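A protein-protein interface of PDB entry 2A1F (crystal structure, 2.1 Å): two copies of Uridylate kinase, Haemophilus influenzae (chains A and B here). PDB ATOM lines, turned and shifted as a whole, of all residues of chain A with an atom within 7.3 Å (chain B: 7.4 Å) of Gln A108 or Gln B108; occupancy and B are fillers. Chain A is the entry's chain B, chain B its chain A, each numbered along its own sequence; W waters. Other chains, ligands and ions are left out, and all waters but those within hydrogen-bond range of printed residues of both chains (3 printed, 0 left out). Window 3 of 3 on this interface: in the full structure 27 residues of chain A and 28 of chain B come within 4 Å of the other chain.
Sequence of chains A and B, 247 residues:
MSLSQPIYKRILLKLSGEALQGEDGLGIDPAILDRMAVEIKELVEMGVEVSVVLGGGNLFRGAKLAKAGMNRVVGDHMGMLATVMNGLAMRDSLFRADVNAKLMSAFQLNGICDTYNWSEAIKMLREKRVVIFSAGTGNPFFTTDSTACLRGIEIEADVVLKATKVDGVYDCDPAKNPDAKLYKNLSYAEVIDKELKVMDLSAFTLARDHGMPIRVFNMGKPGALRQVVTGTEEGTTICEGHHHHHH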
ATOM      1  N   SER A 105      -3.490 -17.358  24.241  1.00  0.00           N
ATOM      2  CA  SER A 105      -4.563 -17.858  25.108  1.00  0.00           C
ATOM      3  C   SER A 105      -4.222 -19.246  25.607  1.00  0.00           C
ATOM      4  O   SER A 105      -3.692 -20.068  24.841  1.00  0.00           O
ATOM      5  CB  SER A 105      -5.884 -17.897  24.327  1.00  0.00           C
ATOM      6  OG  SER A 105      -6.936 -18.407  25.123  1.00  0.00           O
ATOM      7  N   ALA A 106      -4.528 -19.512  26.879  1.00  0.00           N
ATOM      8  CA  ALA A 106      -4.512 -20.876  27.405  1.00  0.00           C
ATOM      9  C   ALA A 106      -5.402 -21.800  26.562  1.00  0.00           C
ATOM     10  O   ALA A 106      -5.027 -22.934  26.308  1.00  0.00           O
ATOM     11  CB  ALA A 106      -4.939 -20.895  28.877  1.00  0.00           C
ATOM     12  N   PHE A 107      -6.537 -21.301  26.084  1.00  0.00           N
ATOM     13  CA  PHE A 107      -7.427 -22.070  25.187  1.00  0.00           C
ATOM     14  C   PHE A 107      -7.097 -21.774  23.761  1.00  0.00           C
ATOM     15  O   PHE A 107      -7.069 -20.617  23.386  1.00  0.00           O
ATOM     16  CB  PHE A 107      -8.916 -21.684  25.285  1.00  0.00           C
ATOM     17  CG  PHE A 107      -9.382 -21.295  26.638  1.00  0.00           C
ATOM     18  CD1 PHE A 107     -10.239 -20.206  26.789  1.00  0.00           C
ATOM     19  CD2 PHE A 107      -9.033 -22.028  27.746  1.00  0.00           C
ATOM     20  CE1 PHE A 107     -10.713 -19.856  28.019  1.00  0.00           C
ATOM     21  CE2 PHE A 107      -9.503 -21.673  28.990  1.00  0.00           C
ATOM     22  CZ  PHE A 107     -10.330 -20.585  29.129  1.00  0.00           C
ATOM     23  N   GLN A 108      -6.894 -22.816  22.963  1.00  0.00           N
ATOM     24  CA  GLN A 108      -6.831 -22.695  21.510  1.00  0.00           C
ATOM     25  C   GLN A 108      -8.093 -22.018  21.021  1.00  0.00           C
ATOM     26  O   GLN A 108      -9.174 -22.498  21.300  1.00  0.00           O
ATOM     27  CB  GLN A 108      -6.748 -24.080  20.890  1.00  0.00           C
ATOM     28  CG  GLN A 108      -6.613 -24.114  19.399  1.00  0.00           C
ATOM     29  CD  GLN A 108      -6.857 -25.512  18.866  1.00  0.00           C
ATOM     30  OE1 GLN A 108      -6.226 -26.477  19.320  1.00  0.00           O
ATOM     31  NE2 GLN A 108      -7.805 -25.638  17.931  1.00  0.00           N
ATOM     32  N   LEU A 109      -7.942 -20.892  20.332  1.00  0.00           N
ATOM     33  CA  LEU A 109      -9.072 -20.104  19.824  1.00  0.00           C
ATOM     34  C   LEU A 109      -8.796 -19.817  18.357  1.00  0.00           C
ATOM     35  O   LEU A 109      -8.309 -18.741  18.010  1.00  0.00           O
ATOM     36  CB  LEU A 109      -9.233 -18.784  20.616  1.00  0.00           C
ATOM     37  CG  LEU A 109      -9.757 -18.901  22.048  1.00  0.00           C
ATOM     38  CD1 LEU A 109      -9.714 -17.595  22.795  1.00  0.00           C
ATOM     39  CD2 LEU A 109     -11.207 -19.425  22.049  1.00  0.00           C
ATOM     40  N   ASN A 110      -9.078 -20.815  17.515  1.00  0.00           N
ATOM     41  CA  ASN A 110      -8.770 -20.755  16.077  1.00  0.00           C
ATOM     42  C   ASN A 110      -9.405 -19.545  15.422  1.00  0.00           C
ATOM     43  O   ASN A 110     -10.605 -19.353  15.536  1.00  0.00           O
ATOM     44  CB  ASN A 110      -9.294 -21.999  15.336  1.00  0.00           C
ATOM     45  CG  ASN A 110      -8.406 -23.219  15.495  1.00  0.00           C
ATOM     46  OD1 ASN A 110      -8.797 -24.333  15.099  1.00  0.00           O
ATOM     47  ND2 ASN A 110      -7.212 -23.030  16.050  1.00  0.00           N
ATOM     48  N   GLY A 111      -8.601 -18.745  14.728  1.00  0.00           N
ATOM     49  CA  GLY A 111      -9.098 -17.545  14.061  1.00  0.00           C
ATOM     50  C   GLY A 111      -9.121 -16.276  14.892  1.00  0.00           C
ATOM     51  O   GLY A 111      -9.399 -15.196  14.374  1.00  0.00           O
ATOM     52  N   ILE A 112      -8.882 -16.406  16.192  1.00  0.00           N
ATOM     53  CA  ILE A 112      -9.006 -15.286  17.100  1.00  0.00           C
ATOM     54  C   ILE A 112      -7.620 -14.806  17.541  1.00  0.00           C
ATOM     55  O   ILE A 112      -7.311 -13.635  17.463  1.00  0.00           O
ATOM     56  CB  ILE A 112      -9.896 -15.650  18.308  1.00  0.00           C
ATOM     57  CG1 ILE A 112     -11.328 -15.874  17.800  1.00  0.00           C
ATOM     58  CG2 ILE A 112      -9.837 -14.560  19.387  1.00  0.00           C
ATOM     59  CD1 ILE A 112     -12.340 -16.088  18.855  1.00  0.00           C
ATOM     60  N   CYS A 113      -6.801 -15.717  18.012  1.00  0.00           N
ATOM     61  CA  CYS A 113      -5.497 -15.344  18.536  1.00  0.00           C
ATOM     62  C   CYS A 113      -4.618 -16.580  18.538  1.00  0.00           C
ATOM     63  O   CYS A 113      -5.068 -17.634  18.087  1.00  0.00           O
ATOM     64  CB  CYS A 113      -5.664 -14.729  19.936  1.00  0.00           C
ATOM     65  SG  CYS A 113      -6.268 -15.846  21.208  1.00  0.00           S
ATOM     66  N   ASP A 114      -3.382 -16.448  19.036  1.00  0.00           N
ATOM     67  CA  ASP A 114      -2.442 -17.552  19.154  1.00  0.00           C
ATOM     68  C   ASP A 114      -2.711 -18.451  20.372  1.00  0.00           C
ATOM     69  O   ASP A 114      -3.237 -17.996  21.381  1.00  0.00           O
ATOM     70  CB  ASP A 114      -1.010 -16.998  19.302  1.00  0.00           C
ATOM     71  CG  ASP A 114      -0.301 -16.838  17.981  1.00  0.00           C
ATOM     72  OD1 ASP A 114      -0.765 -16.034  17.129  1.00  0.00           O
ATOM     73  OD2 ASP A 114       0.741 -17.508  17.805  1.00  0.00           O
ATOM     74  N   THR A 115      -2.298 -19.715  20.297  1.00  0.00           N
ATOM     75  CA  THR A 115      -2.322 -20.607  21.470  1.00  0.00           C
ATOM     76  C   THR A 115      -1.032 -20.453  22.302  1.00  0.00           C
ATOM     77  O   THR A 115       0.055 -20.340  21.750  1.00  0.00           O
ATOM     78  CB  THR A 115      -2.465 -22.061  21.071  1.00  0.00           C
ATOM     79  OG1 THR A 115      -3.587 -22.207  20.192  1.00  0.00           O
ATOM     80  CG2 THR A 115      -2.675 -22.943  22.320  1.00  0.00           C
ATOM     81  N   TYR A 116      -1.157 -20.431  23.622  1.00  0.00           N
ATOM     82  CA  TYR A 116       0.010 -20.214  24.459  1.00  0.00           C
ATOM     83  C   TYR A 116       1.003 -21.366  24.347  1.00  0.00           C
ATOM     84  O   TYR A 116       0.649 -22.558  24.391  1.00  0.00           O
ATOM     85  CB  TYR A 116      -0.330 -19.971  25.927  1.00  0.00           C
ATOM     86  CG  TYR A 116       0.925 -19.844  26.786  1.00  0.00           C
ATOM     87  CD1 TYR A 116       1.661 -18.674  26.799  1.00  0.00           C
ATOM     88  CD2 TYR A 116       1.390 -20.899  27.539  1.00  0.00           C
ATOM     89  CE1 TYR A 116       2.820 -18.545  27.568  1.00  0.00           C
ATOM     90  CE2 TYR A 116       2.545 -20.775  28.313  1.00  0.00           C
ATOM     91  CZ  TYR A 116       3.247 -19.594  28.320  1.00  0.00           C
ATOM     92  OH  TYR A 116       4.384 -19.449  29.089  1.00  0.00           O
ATOM     93  N   SER B 105     -20.428 -24.523  21.289  1.00  0.00           N
ATOM     94  CA  SER B 105     -19.747 -23.309  20.832  1.00  0.00           C
ATOM     95  C   SER B 105     -19.252 -23.506  19.401  1.00  0.00           C
ATOM     96  O   SER B 105     -18.816 -24.595  19.044  1.00  0.00           O
ATOM     97  CB  SER B 105     -18.555 -23.020  21.762  1.00  0.00           C
ATOM     98  OG  SER B 105     -17.781 -21.945  21.286  1.00  0.00           O
ATOM     99  N   ALA B 106     -19.323 -22.454  18.590  1.00  0.00           N
ATOM    100  CA  ALA B 106     -18.649 -22.439  17.305  1.00  0.00           C
ATOM    101  C   ALA B 106     -17.118 -22.627  17.442  1.00  0.00           C
ATOM    102  O   ALA B 106     -16.508 -23.203  16.568  1.00  0.00           O
ATOM    103  CB  ALA B 106     -18.965 -21.162  16.580  1.00  0.00           C
ATOM    104  N   PHE B 107     -16.495 -22.180  18.532  1.00  0.00           N
ATOM    105  CA  PHE B 107     -15.073 -22.469  18.752  1.00  0.00           C
ATOM    106  C   PHE B 107     -14.961 -23.656  19.680  1.00  0.00           C
ATOM    107  O   PHE B 107     -15.595 -23.672  20.734  1.00  0.00           O
ATOM    108  CB  PHE B 107     -14.264 -21.355  19.462  1.00  0.00           C
ATOM    109  CG  PHE B 107     -14.789 -19.974  19.294  1.00  0.00           C
ATOM    110  CD1 PHE B 107     -14.979 -19.163  20.417  1.00  0.00           C
ATOM    111  CD2 PHE B 107     -15.022 -19.455  18.051  1.00  0.00           C
ATOM    112  CE1 PHE B 107     -15.423 -17.872  20.294  1.00  0.00           C
ATOM    113  CE2 PHE B 107     -15.478 -18.163  17.906  1.00  0.00           C
ATOM    114  CZ  PHE B 107     -15.679 -17.369  19.031  1.00  0.00           C
ATOM    115  N   GLN B 108     -14.116 -24.606  19.319  1.00  0.00           N
ATOM    116  CA  GLN B 108     -13.733 -25.670  20.214  1.00  0.00           C
ATOM    117  C   GLN B 108     -13.182 -24.982  21.461  1.00  0.00           C
ATOM    118  O   GLN B 108     -12.297 -24.145  21.353  1.00  0.00           O
ATOM    119  CB  GLN B 108     -12.684 -26.523  19.511  1.00  0.00           C
ATOM    120  CG  GLN B 108     -11.985 -27.590  20.311  1.00  0.00           C
ATOM    121  CD  GLN B 108     -10.680 -27.958  19.633  1.00  0.00           C
ATOM    122  OE1 GLN B 108     -10.676 -28.295  18.445  1.00  0.00           O
ATOM    123  NE2 GLN B 108      -9.559 -27.849  20.363  1.00  0.00           N
ATOM    124  N   LEU B 109     -13.794 -25.259  22.612  1.00  0.00           N
ATOM    125  CA  LEU B 109     -13.374 -24.688  23.906  1.00  0.00           C
ATOM    126  C   LEU B 109     -13.168 -25.863  24.857  1.00  0.00           C
ATOM    127  O   LEU B 109     -14.055 -26.234  25.631  1.00  0.00           O
ATOM    128  CB  LEU B 109     -14.400 -23.682  24.457  1.00  0.00           C
ATOM    129  CG  LEU B 109     -14.529 -22.303  23.786  1.00  0.00           C
ATOM    130  CD1 LEU B 109     -15.666 -21.539  24.395  1.00  0.00           C
ATOM    131  CD2 LEU B 109     -13.246 -21.465  23.917  1.00  0.00           C
ATOM    132  N   ASN B 110     -11.982 -26.461  24.745  1.00  0.00           N
ATOM    133  CA  ASN B 110     -11.642 -27.704  25.446  1.00  0.00           C
ATOM    134  C   ASN B 110     -11.727 -27.514  26.944  1.00  0.00           C
ATOM    135  O   ASN B 110     -11.058 -26.653  27.488  1.00  0.00           O
ATOM    136  CB  ASN B 110     -10.204 -28.147  25.090  1.00  0.00           C
ATOM    137  CG  ASN B 110     -10.134 -29.031  23.853  1.00  0.00           C
ATOM    138  OD1 ASN B 110      -9.034 -29.397  23.408  1.00  0.00           O
ATOM    139  ND2 ASN B 110     -11.286 -29.393  23.305  1.00  0.00           N
ATOM    140  N   GLY B 111     -12.558 -28.307  27.598  1.00  0.00           N
ATOM    141  CA  GLY B 111     -12.706 -28.227  29.040  1.00  0.00           C
ATOM    142  C   GLY B 111     -13.839 -27.340  29.520  1.00  0.00           C
ATOM    143  O   GLY B 111     -14.172 -27.381  30.690  1.00  0.00           O
ATOM    144  N   ILE B 112     -14.409 -26.534  28.625  1.00  0.00           N
ATOM    145  CA  ILE B 112     -15.438 -25.545  28.986  1.00  0.00           C
ATOM    146  C   ILE B 112     -16.812 -26.023  28.507  1.00  0.00           C
ATOM    147  O   ILE B 112     -17.773 -26.023  29.273  1.00  0.00           O
ATOM    148  CB  ILE B 112     -15.103 -24.138  28.421  1.00  0.00           C
ATOM    149  CG1 ILE B 112     -13.830 -23.591  29.106  1.00  0.00           C
ATOM    150  CG2 ILE B 112     -16.255 -23.145  28.633  1.00  0.00           C
ATOM    151  CD1 ILE B 112     -13.250 -22.414  28.431  1.00  0.00           C
ATOM    152  N   CYS B 113     -16.900 -26.415  27.242  1.00  0.00           N
ATOM    153  CA  CYS B 113     -18.154 -26.889  26.676  1.00  0.00           C
ATOM    154  C   CYS B 113     -17.930 -27.733  25.415  1.00  0.00           C
ATOM    155  O   CYS B 113     -16.776 -27.973  25.016  1.00  0.00           O
ATOM    156  CB  CYS B 113     -19.038 -25.686  26.384  1.00  0.00           C
ATOM    157  SG  CYS B 113     -18.413 -24.586  25.095  1.00  0.00           S
ATOM    158  N   ASP B 114     -19.034 -28.159  24.786  1.00  0.00           N
ATOM    159  CA  ASP B 114     -18.998 -28.919  23.539  1.00  0.00           C
ATOM    160  C   ASP B 114     -18.711 -28.079  22.308  1.00  0.00           C
ATOM    161  O   ASP B 114     -19.054 -26.918  22.252  1.00  0.00           O
ATOM    162  CB  ASP B 114     -20.356 -29.600  23.301  1.00  0.00           C
ATOM    163  CG  ASP B 114     -20.540 -30.838  24.137  1.00  0.00           C
ATOM    164  OD1 ASP B 114     -20.495 -30.743  25.392  1.00  0.00           O
ATOM    165  OD2 ASP B 114     -20.755 -31.916  23.529  1.00  0.00           O
ATOM    166  N   THR B 115     -18.118 -28.688  21.288  1.00  0.00           N
ATOM    167  CA  THR B 115     -18.002 -28.024  20.001  1.00  0.00           C
ATOM    168  C   THR B 115     -19.284 -28.250  19.209  1.00  0.00           C
ATOM    169  O   THR B 115     -19.863 -29.322  19.270  1.00  0.00           O
ATOM    170  CB  THR B 115     -16.814 -28.553  19.188  1.00  0.00           C
ATOM    171  OG1 THR B 115     -15.652 -28.566  20.013  1.00  0.00           O
ATOM    172  CG2 THR B 115     -16.566 -27.654  17.994  1.00  0.00           C
ATOM    173  N   TYR B 116     -19.735 -27.229  18.495  1.00  0.00           N
ATOM    174  CA  TYR B 116     -20.939 -27.345  17.690  1.00  0.00           C
ATOM    175  C   TYR B 116     -20.777 -28.340  16.527  1.00  0.00           C
ATOM    176  O   TYR B 116     -19.773 -28.346  15.787  1.00  0.00           O
ATOM    177  CB  TYR B 116     -21.415 -25.992  17.144  1.00  0.00           C
ATOM    178  CG  TYR B 116     -22.643 -26.135  16.247  1.00  0.00           C
ATOM    179  CD1 TYR B 116     -23.887 -26.416  16.791  1.00  0.00           C
ATOM    180  CD2 TYR B 116     -22.548 -26.053  14.868  1.00  0.00           C
ATOM    181  CE1 TYR B 116     -25.008 -26.576  15.988  1.00  0.00           C
ATOM    182  CE2 TYR B 116     -23.666 -26.206  14.064  1.00  0.00           C
ATOM    183  CZ  TYR B 116     -24.886 -26.470  14.621  1.00  0.00           C
ATOM    184  OH  TYR B 116     -26.013 -26.605  13.827  1.00  0.00           O
HETATM  185  O   HOH W   1      -7.824 -28.866  18.112  1.00  0.00           O
HETATM  186  O   HOH W   2     -10.218 -25.058  22.610  1.00  0.00           O
HETATM  187  O   HOH W   3     -10.356 -23.236  18.769  1.00  0.00           O
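Ala A106 touches none of the printed residues of chain B. Of the printed residues of chain B, Phe A107 touches Ile B112 (3.5 Å). Gln A108 touches just one residue of chain B: Gln B108 (3.5 Å). Printed residues of chain B within 4 Å of Leu A109: Leu B109 (3.4 Å). Of chain A, only Gln A108 comes within 4 Å of Gln B108. The nearest residue of chain B that does not touch Gln A108 is Leu B109 (4.9 Å). The nearest residue of chain A that does not touch Gln B108 is Leu A109 (4.9 Å). The nearest printed residue of chain B that does not touch Leu A109 is Phe B107 (4.1 Å).
Printed residues of chain B that touch a printed residue of chain A: Phe B107, Gln B108, Leu B109 and Ile B112. Hydrophobic or aromatic side chains of chain B that line the printed part of chain A: Phe B107, Leu B109 and Ile B112.
Phe A107 touches Ile B112, and with the chains exchanged Ile A112 touches Phe B107. Gln A108 touches its own counterpart, Gln B108. Leu A109 touches its own counterpart, Leu B109. Of the 4 pairs that touch across the chains among the printed residues, 4 have their exchanged pair printed and touching as well.
The backbone carbonyl oxygen (O) of Phe B107 sits at hydrogen-bond distance from the side-chain hydroxyl (OG) of Ser B105, 2.8 Å away. O of Phe A107 sits at hydrogen-bond distance from OG of Ser A105. NE2 of Gln B108 sits at hydrogen-bond distance from OD1 of Asn B110. The side-chain amide nitrogen (NE2) of Gln A108 sits close to the side-chain amide nitrogen (ND2) of Asn A110, 3.3 Å away.
Phe A107 touches Ile B112 (CZ to CD1, 3.5 Å). Gln A108 touches Gln B108. CD2 of Leu A109 touches CD2 of Leu B109, at 3.4 Å. CD1 of Ile A112 touches CZ of Phe B107, at 3.6 Å.
Water W2 lies within hydrogen-bond range of the backbone carbonyl oxygen of Gln B108, the backbone carbonyl oxygen of Gln A108 and the backbone NH of Asn B110. Water W3 lies within hydrogen-bond range of O of Gln A108 (2.9 Å), N of Asn A110 (3.0 Å) and O of Gln B108 (3.4 Å). Water W1 lies within hydrogen-bond range of the side-chain amide oxygen (OE1) of Gln B108 and the side-chain amide oxygen (OE1) of Gln A108.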
